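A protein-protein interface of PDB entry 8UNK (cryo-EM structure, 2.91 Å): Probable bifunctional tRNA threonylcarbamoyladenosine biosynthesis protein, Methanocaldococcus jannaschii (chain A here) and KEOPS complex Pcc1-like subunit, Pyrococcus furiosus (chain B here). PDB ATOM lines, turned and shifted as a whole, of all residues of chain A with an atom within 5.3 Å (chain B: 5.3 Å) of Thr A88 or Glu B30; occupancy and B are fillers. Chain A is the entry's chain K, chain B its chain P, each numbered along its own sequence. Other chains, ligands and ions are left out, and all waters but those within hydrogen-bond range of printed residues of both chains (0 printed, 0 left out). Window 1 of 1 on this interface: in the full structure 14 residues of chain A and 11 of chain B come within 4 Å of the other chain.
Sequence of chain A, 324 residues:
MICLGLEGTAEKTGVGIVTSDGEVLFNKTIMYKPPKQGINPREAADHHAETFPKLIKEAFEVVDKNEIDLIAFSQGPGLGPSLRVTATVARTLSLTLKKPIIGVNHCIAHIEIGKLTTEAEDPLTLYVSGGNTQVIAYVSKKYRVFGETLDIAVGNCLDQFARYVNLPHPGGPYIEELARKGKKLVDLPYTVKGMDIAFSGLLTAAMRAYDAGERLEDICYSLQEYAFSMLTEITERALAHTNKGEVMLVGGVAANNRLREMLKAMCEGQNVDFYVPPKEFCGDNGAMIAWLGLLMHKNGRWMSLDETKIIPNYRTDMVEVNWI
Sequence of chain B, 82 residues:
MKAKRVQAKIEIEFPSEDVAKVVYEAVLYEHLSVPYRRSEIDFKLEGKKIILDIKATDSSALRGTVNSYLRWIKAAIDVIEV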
ATOM      1  N   LEU A  83      26.551  11.820  23.913  1.00  0.00           N
ATOM      2  CA  LEU A  83      27.237  13.073  23.631  1.00  0.00           C
ATOM      3  C   LEU A  83      26.677  14.199  24.489  1.00  0.00           C
ATOM      4  O   LEU A  83      27.424  15.064  24.959  1.00  0.00           O
ATOM      5  CB  LEU A  83      27.121  13.405  22.146  1.00  0.00           C
ATOM      6  CG  LEU A  83      27.995  12.536  21.244  1.00  0.00           C
ATOM      7  CD1 LEU A  83      27.712  12.827  19.785  1.00  0.00           C
ATOM      8  CD2 LEU A  83      29.458  12.746  21.571  1.00  0.00           C
ATOM      9  N   ARG A  84      25.361  14.196  24.717  1.00  0.00           N
ATOM     10  CA  ARG A  84      24.757  15.191  25.598  1.00  0.00           C
ATOM     11  C   ARG A  84      25.369  15.124  26.990  1.00  0.00           C
ATOM     12  O   ARG A  84      25.755  16.148  27.566  1.00  0.00           O
ATOM     13  CB  ARG A  84      23.246  14.967  25.679  1.00  0.00           C
ATOM     14  CG  ARG A  84      22.461  15.557  24.527  1.00  0.00           C
ATOM     15  CD  ARG A  84      20.964  15.488  24.782  1.00  0.00           C
ATOM     16  NE  ARG A  84      20.221  15.210  23.559  1.00  0.00           N
ATOM     17  CZ  ARG A  84      20.157  16.028  22.518  1.00  0.00           C
ATOM     18  NH1 ARG A  84      20.757  17.207  22.525  1.00  0.00           N
ATOM     19  NH2 ARG A  84      19.473  15.654  21.440  1.00  0.00           N
ATOM     20  N   VAL A  85      25.458  13.915  27.547  1.00  0.00           N
ATOM     21  CA  VAL A  85      25.943  13.764  28.914  1.00  0.00           C
ATOM     22  C   VAL A  85      27.413  14.152  29.009  1.00  0.00           C
ATOM     23  O   VAL A  85      27.820  14.865  29.935  1.00  0.00           O
ATOM     24  CB  VAL A  85      25.699  12.330  29.414  1.00  0.00           C
ATOM     25  CG1 VAL A  85      26.505  12.067  30.671  1.00  0.00           C
ATOM     26  CG2 VAL A  85      24.218  12.116  29.680  1.00  0.00           C
ATOM     27  N   THR A  86      28.238  13.697  28.062  1.00  0.00           N
ATOM     28  CA  THR A  86      29.648  14.071  28.114  1.00  0.00           C
ATOM     29  C   THR A  86      29.819  15.576  27.958  1.00  0.00           C
ATOM     30  O   THR A  86      30.642  16.186  28.650  1.00  0.00           O
ATOM     31  CB  THR A  86      30.459  13.331  27.050  1.00  0.00           C
ATOM     32  OG1 THR A  86      31.835  13.719  27.145  1.00  0.00           O
ATOM     33  CG2 THR A  86      29.965  13.655  25.671  1.00  0.00           C
ATOM     34  N   ALA A  87      29.043  16.199  27.067  1.00  0.00           N
ATOM     35  CA  ALA A  87      29.164  17.637  26.858  1.00  0.00           C
ATOM     36  C   ALA A  87      28.760  18.415  28.103  1.00  0.00           C
ATOM     37  O   ALA A  87      29.445  19.364  28.498  1.00  0.00           O
ATOM     38  CB  ALA A  87      28.315  18.059  25.659  1.00  0.00           C
ATOM     39  N   THR A  88      27.648  18.034  28.736  1.00  0.00           N
ATOM     40  CA  THR A  88      27.217  18.754  29.932  1.00  0.00           C
ATOM     41  C   THR A  88      28.198  18.549  31.081  1.00  0.00           C
ATOM     42  O   THR A  88      28.480  19.488  31.833  1.00  0.00           O
ATOM     43  CB  THR A  88      25.807  18.330  30.347  1.00  0.00           C
ATOM     44  OG1 THR A  88      25.414  19.057  31.516  1.00  0.00           O
ATOM     45  CG2 THR A  88      25.741  16.851  30.649  1.00  0.00           C
ATOM     46  N   VAL A  89      28.731  17.334  31.233  1.00  0.00           N
ATOM     47  CA  VAL A  89      29.719  17.097  32.282  1.00  0.00           C
ATOM     48  C   VAL A  89      30.969  17.931  32.034  1.00  0.00           C
ATOM     49  O   VAL A  89      31.527  18.530  32.962  1.00  0.00           O
ATOM     50  CB  VAL A  89      30.050  15.596  32.372  1.00  0.00           C
ATOM     51  N   ALA A  90      31.432  17.984  30.784  1.00  0.00           N
ATOM     52  CA  ALA A  90      32.606  18.788  30.474  1.00  0.00           C
ATOM     53  C   ALA A  90      32.345  20.265  30.725  1.00  0.00           C
ATOM     54  O   ALA A  90      33.217  20.979  31.232  1.00  0.00           O
ATOM     55  CB  ALA A  90      33.026  18.557  29.025  1.00  0.00           C
ATOM     56  N   ARG A  91      31.155  20.750  30.362  1.00  0.00           N
ATOM     57  CA  ARG A  91      30.824  22.149  30.617  1.00  0.00           C
ATOM     58  C   ARG A  91      30.813  22.440  32.111  1.00  0.00           C
ATOM     59  O   ARG A  91      31.331  23.472  32.555  1.00  0.00           O
ATOM     60  CB  ARG A  91      29.468  22.491  29.998  1.00  0.00           C
ATOM     61  CG  ARG A  91      29.527  22.871  28.524  1.00  0.00           C
ATOM     62  CD  ARG A  91      28.152  23.263  28.002  1.00  0.00           C
ATOM     63  NE  ARG A  91      27.754  22.468  26.844  1.00  0.00           N
ATOM     64  CZ  ARG A  91      26.756  21.593  26.836  1.00  0.00           C
ATOM     65  NH1 ARG A  91      26.022  21.368  27.914  1.00  0.00           N
ATOM     66  NH2 ARG A  91      26.488  20.926  25.718  1.00  0.00           N
ATOM     67  N   THR A  92      30.221  21.544  32.903  1.00  0.00           N
ATOM     68  CA  THR A  92      30.208  21.739  34.347  1.00  0.00           C
ATOM     69  C   THR A  92      31.625  21.772  34.900  1.00  0.00           C
ATOM     70  O   THR A  92      31.951  22.620  35.738  1.00  0.00           O
ATOM     71  CB  THR A  92      29.396  20.631  35.023  1.00  0.00           C
ATOM     72  OG1 THR A  92      28.114  20.519  34.393  1.00  0.00           O
ATOM     73  CG2 THR A  92      29.202  20.933  36.498  1.00  0.00           C
ATOM     74  N   LEU A  93      32.485  20.864  34.436  1.00  0.00           N
ATOM     75  CA  LEU A  93      33.874  20.866  34.887  1.00  0.00           C
ATOM     76  C   LEU A  93      34.562  22.176  34.530  1.00  0.00           C
ATOM     77  O   LEU A  93      35.242  22.784  35.364  1.00  0.00           O
ATOM     78  CB  LEU A  93      34.629  19.685  34.271  1.00  0.00           C
ATOM     79  CG  LEU A  93      34.924  18.493  35.182  1.00  0.00           C
ATOM     80  CD1 LEU A  93      36.024  18.838  36.173  1.00  0.00           C
ATOM     81  CD2 LEU A  93      33.672  18.039  35.903  1.00  0.00           C
ATOM     82  N   ALA B  26      23.720  25.269  34.070  1.00  0.00           N
ATOM     83  CA  ALA B  26      24.382  24.143  33.420  1.00  0.00           C
ATOM     84  C   ALA B  26      23.456  23.333  32.521  1.00  0.00           C
ATOM     85  O   ALA B  26      23.909  22.805  31.499  1.00  0.00           O
ATOM     86  CB  ALA B  26      24.995  23.220  34.476  1.00  0.00           C
ATOM     87  N   VAL B  27      22.173  23.219  32.870  1.00  0.00           N
ATOM     88  CA  VAL B  27      21.264  22.324  32.154  1.00  0.00           C
ATOM     89  C   VAL B  27      20.474  23.070  31.083  1.00  0.00           C
ATOM     90  O   VAL B  27      20.223  22.531  29.997  1.00  0.00           O
ATOM     91  CB  VAL B  27      20.309  21.620  33.134  1.00  0.00           C
ATOM     92  CG1 VAL B  27      19.308  20.759  32.376  1.00  0.00           C
ATOM     93  CG2 VAL B  27      21.091  20.781  34.131  1.00  0.00           C
ATOM     94  N   LEU B  28      20.059  24.306  31.378  1.00  0.00           N
ATOM     95  CA  LEU B  28      19.250  25.056  30.424  1.00  0.00           C
ATOM     96  C   LEU B  28      19.954  25.194  29.083  1.00  0.00           C
ATOM     97  O   LEU B  28      19.293  25.321  28.046  1.00  0.00           O
ATOM     98  CB  LEU B  28      18.918  26.436  30.990  1.00  0.00           C
ATOM     99  N   TYR B  29      21.289  25.175  29.078  1.00  0.00           N
ATOM    100  CA  TYR B  29      22.013  25.180  27.813  1.00  0.00           C
ATOM    101  C   TYR B  29      21.708  23.926  27.004  1.00  0.00           C
ATOM    102  O   TYR B  29      21.499  23.999  25.788  1.00  0.00           O
ATOM    103  CB  TYR B  29      23.513  25.302  28.068  1.00  0.00           C
ATOM    104  CG  TYR B  29      24.328  25.454  26.807  1.00  0.00           C
ATOM    105  CD1 TYR B  29      24.462  24.402  25.913  1.00  0.00           C
ATOM    106  CD2 TYR B  29      24.960  26.650  26.506  1.00  0.00           C
ATOM    107  CE1 TYR B  29      25.195  24.532  24.765  1.00  0.00           C
ATOM    108  CE2 TYR B  29      25.700  26.789  25.356  1.00  0.00           C
ATOM    109  CZ  TYR B  29      25.813  25.725  24.489  1.00  0.00           C
ATOM    110  OH  TYR B  29      26.548  25.843  23.336  1.00  0.00           O
ATOM    111  N   GLU B  30      21.694  22.763  27.655  1.00  0.00           N
ATOM    112  CA  GLU B  30      21.327  21.540  26.949  1.00  0.00           C
ATOM    113  C   GLU B  30      19.867  21.583  26.523  1.00  0.00           C
ATOM    114  O   GLU B  30      19.500  21.040  25.475  1.00  0.00           O
ATOM    115  CB  GLU B  30      21.591  20.320  27.830  1.00  0.00           C
ATOM    116  CG  GLU B  30      21.783  19.029  27.050  1.00  0.00           C
ATOM    117  CD  GLU B  30      21.639  17.793  27.916  1.00  0.00           C
ATOM    118  OE1 GLU B  30      22.323  17.707  28.958  1.00  0.00           O
ATOM    119  OE2 GLU B  30      20.841  16.904  27.554  1.00  0.00           O
ATOM    120  N   HIS B  31      19.018  22.226  27.327  1.00  0.00           N
ATOM    121  CA  HIS B  31      17.604  22.321  26.978  1.00  0.00           C
ATOM    122  C   HIS B  31      17.406  23.067  25.664  1.00  0.00           C
ATOM    123  O   HIS B  31      16.571  22.676  24.840  1.00  0.00           O
ATOM    124  CB  HIS B  31      16.830  23.012  28.099  1.00  0.00           C
ATOM    125  CG  HIS B  31      15.588  23.706  27.635  1.00  0.00           C
ATOM    126  ND1 HIS B  31      14.483  23.025  27.172  1.00  0.00           N
ATOM    127  CD2 HIS B  31      15.278  25.021  27.555  1.00  0.00           C
ATOM    128  CE1 HIS B  31      13.545  23.890  26.832  1.00  0.00           C
ATOM    129  NE2 HIS B  31      14.003  25.109  27.055  1.00  0.00           N
ATOM    130  N   LEU B  32      18.162  24.141  25.449  1.00  0.00           N
ATOM    131  CA  LEU B  32      17.976  24.993  24.281  1.00  0.00           C
ATOM    132  C   LEU B  32      18.627  24.432  23.021  1.00  0.00           C
ATOM    133  O   LEU B  32      18.556  25.077  21.970  1.00  0.00           O
ATOM    134  CB  LEU B  32      18.506  26.402  24.576  1.00  0.00           C
ATOM    135  CG  LEU B  32      20.003  26.696  24.429  1.00  0.00           C
ATOM    136  CD1 LEU B  32      20.419  26.942  22.982  1.00  0.00           C
ATOM    137  CD2 LEU B  32      20.379  27.888  25.298  1.00  0.00           C
ATOM    138  N   SER B  33      19.246  23.254  23.092  1.00  0.00           N
ATOM    139  CA  SER B  33      19.830  22.605  21.924  1.00  0.00           C
ATOM    140  C   SER B  33      18.850  21.653  21.244  1.00  0.00           C
ATOM    141  O   SER B  33      19.206  21.005  20.255  1.00  0.00           O
ATOM    142  CB  SER B  33      21.104  21.857  22.316  1.00  0.00           C
ATOM    143  OG  SER B  33      22.130  22.758  22.699  1.00  0.00           O
ATOM    144  N   VAL B  34      17.627  21.553  21.757  1.00  0.00           N
ATOM    145  CA  VAL B  34      16.586  20.721  21.157  1.00  0.00           C
ATOM    146  C   VAL B  34      15.371  21.601  20.883  1.00  0.00           C
ATOM    147  O   VAL B  34      14.640  21.948  21.823  1.00  0.00           O
ATOM    148  CB  VAL B  34      16.223  19.538  22.069  1.00  0.00           C
ATOM    149  CG1 VAL B  34      15.277  18.586  21.353  1.00  0.00           C
ATOM    150  CG2 VAL B  34      17.480  18.812  22.520  1.00  0.00           C
ATOM    151  N   TRP B  72      19.414  14.827  33.392  1.00  0.00           N
ATOM    152  CA  TRP B  72      20.355  15.906  33.107  1.00  0.00           C
ATOM    153  C   TRP B  72      20.675  16.694  34.371  1.00  0.00           C
ATOM    154  O   TRP B  72      21.847  16.953  34.675  1.00  0.00           O
ATOM    155  CB  TRP B  72      19.783  16.837  32.038  1.00  0.00           C
ATOM    156  CG  TRP B  72      19.387  16.151  30.765  1.00  0.00           C
ATOM    157  CD1 TRP B  72      19.666  14.867  30.399  1.00  0.00           C
ATOM    158  CD2 TRP B  72      18.628  16.717  29.690  1.00  0.00           C
ATOM    159  NE1 TRP B  72      19.130  14.599  29.163  1.00  0.00           N
ATOM    160  CE2 TRP B  72      18.488  15.719  28.707  1.00  0.00           C
ATOM    161  CE3 TRP B  72      18.057  17.972  29.464  1.00  0.00           C
ATOM    162  CZ2 TRP B  72      17.804  15.938  27.516  1.00  0.00           C
ATOM    163  CZ3 TRP B  72      17.376  18.186  28.281  1.00  0.00           C
ATOM    164  CH2 TRP B  72      17.254  17.174  27.323  1.00  0.00           C
ATOM    165  N   ALA B  75      22.872  14.388  36.820  1.00  0.00           N
ATOM    166  CA  ALA B  75      24.247  14.385  36.333  1.00  0.00           C
ATOM    167  C   ALA B  75      24.933  15.713  36.618  1.00  0.00           C
ATOM    168  O   ALA B  75      26.045  15.740  37.155  1.00  0.00           O
ATOM    169  CB  ALA B  75      24.272  14.083  34.836  1.00  0.00           C
ATOM    170  N   ALA B  76      24.264  16.828  36.314  1.00  0.00           N
ATOM    171  CA  ALA B  76      24.883  18.135  36.497  1.00  0.00           C
ATOM    172  C   ALA B  76      25.261  18.370  37.955  1.00  0.00           C
ATOM    173  O   ALA B  76      26.369  18.833  38.252  1.00  0.00           O
ATOM    174  CB  ALA B  76      23.939  19.230  36.003  1.00  0.00           C
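The backbone carbonyl oxygen (O) of Thr A88 sits at hydrogen-bond distance from the side-chain hydroxyl (OG1) of Thr A92.
O of Tyr B29 sits at hydrogen-bond distance from OG of Ser B33 (3.4 Å).
NE1 of Trp B72 lies close to OE2 of Glu B30, at 3.3 Å.
OE2 of Glu B30 touches CD of Arg A84 (3.1 Å).
CG2 of Val B34 touches NH1 of Arg A84, at 3.6 Å.
Thr A88 touches Glu B30 (CB to OE1, 3.8 Å).
Tyr B29 touches Arg A91 (CD1 to CZ, 3.7 Å).
Thr A92 touches Ala B76 (CG2 to O, 3.9 Å).
Of chain B, only Glu B30 comes within 4 Å of Thr A88.
Printed residues of chain B within 4 Å of Arg A91: Tyr B29.
Of the printed residues of chain B, Thr A92 touches Ala B76 (3.9 Å).
The nearest residue of chain A that does not touch Glu B30 is Arg A91 (4.6 Å).
Of the 11 printed residues of chain A, 4 touch a printed residue of chain B.
Of the 12 printed residues of chain B, 4 touch a printed residue of chain A.
Printed residues of chain B that touch a printed residue of chain A: Tyr B29, Glu B30, Val B34 and Ala B76.
Hydrophobic or aromatic side chains of chain B within 4 Å of the printed part of chain A: Tyr B29 and Val B34.
Among the printed residues, 5 pairs touch across the chains.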
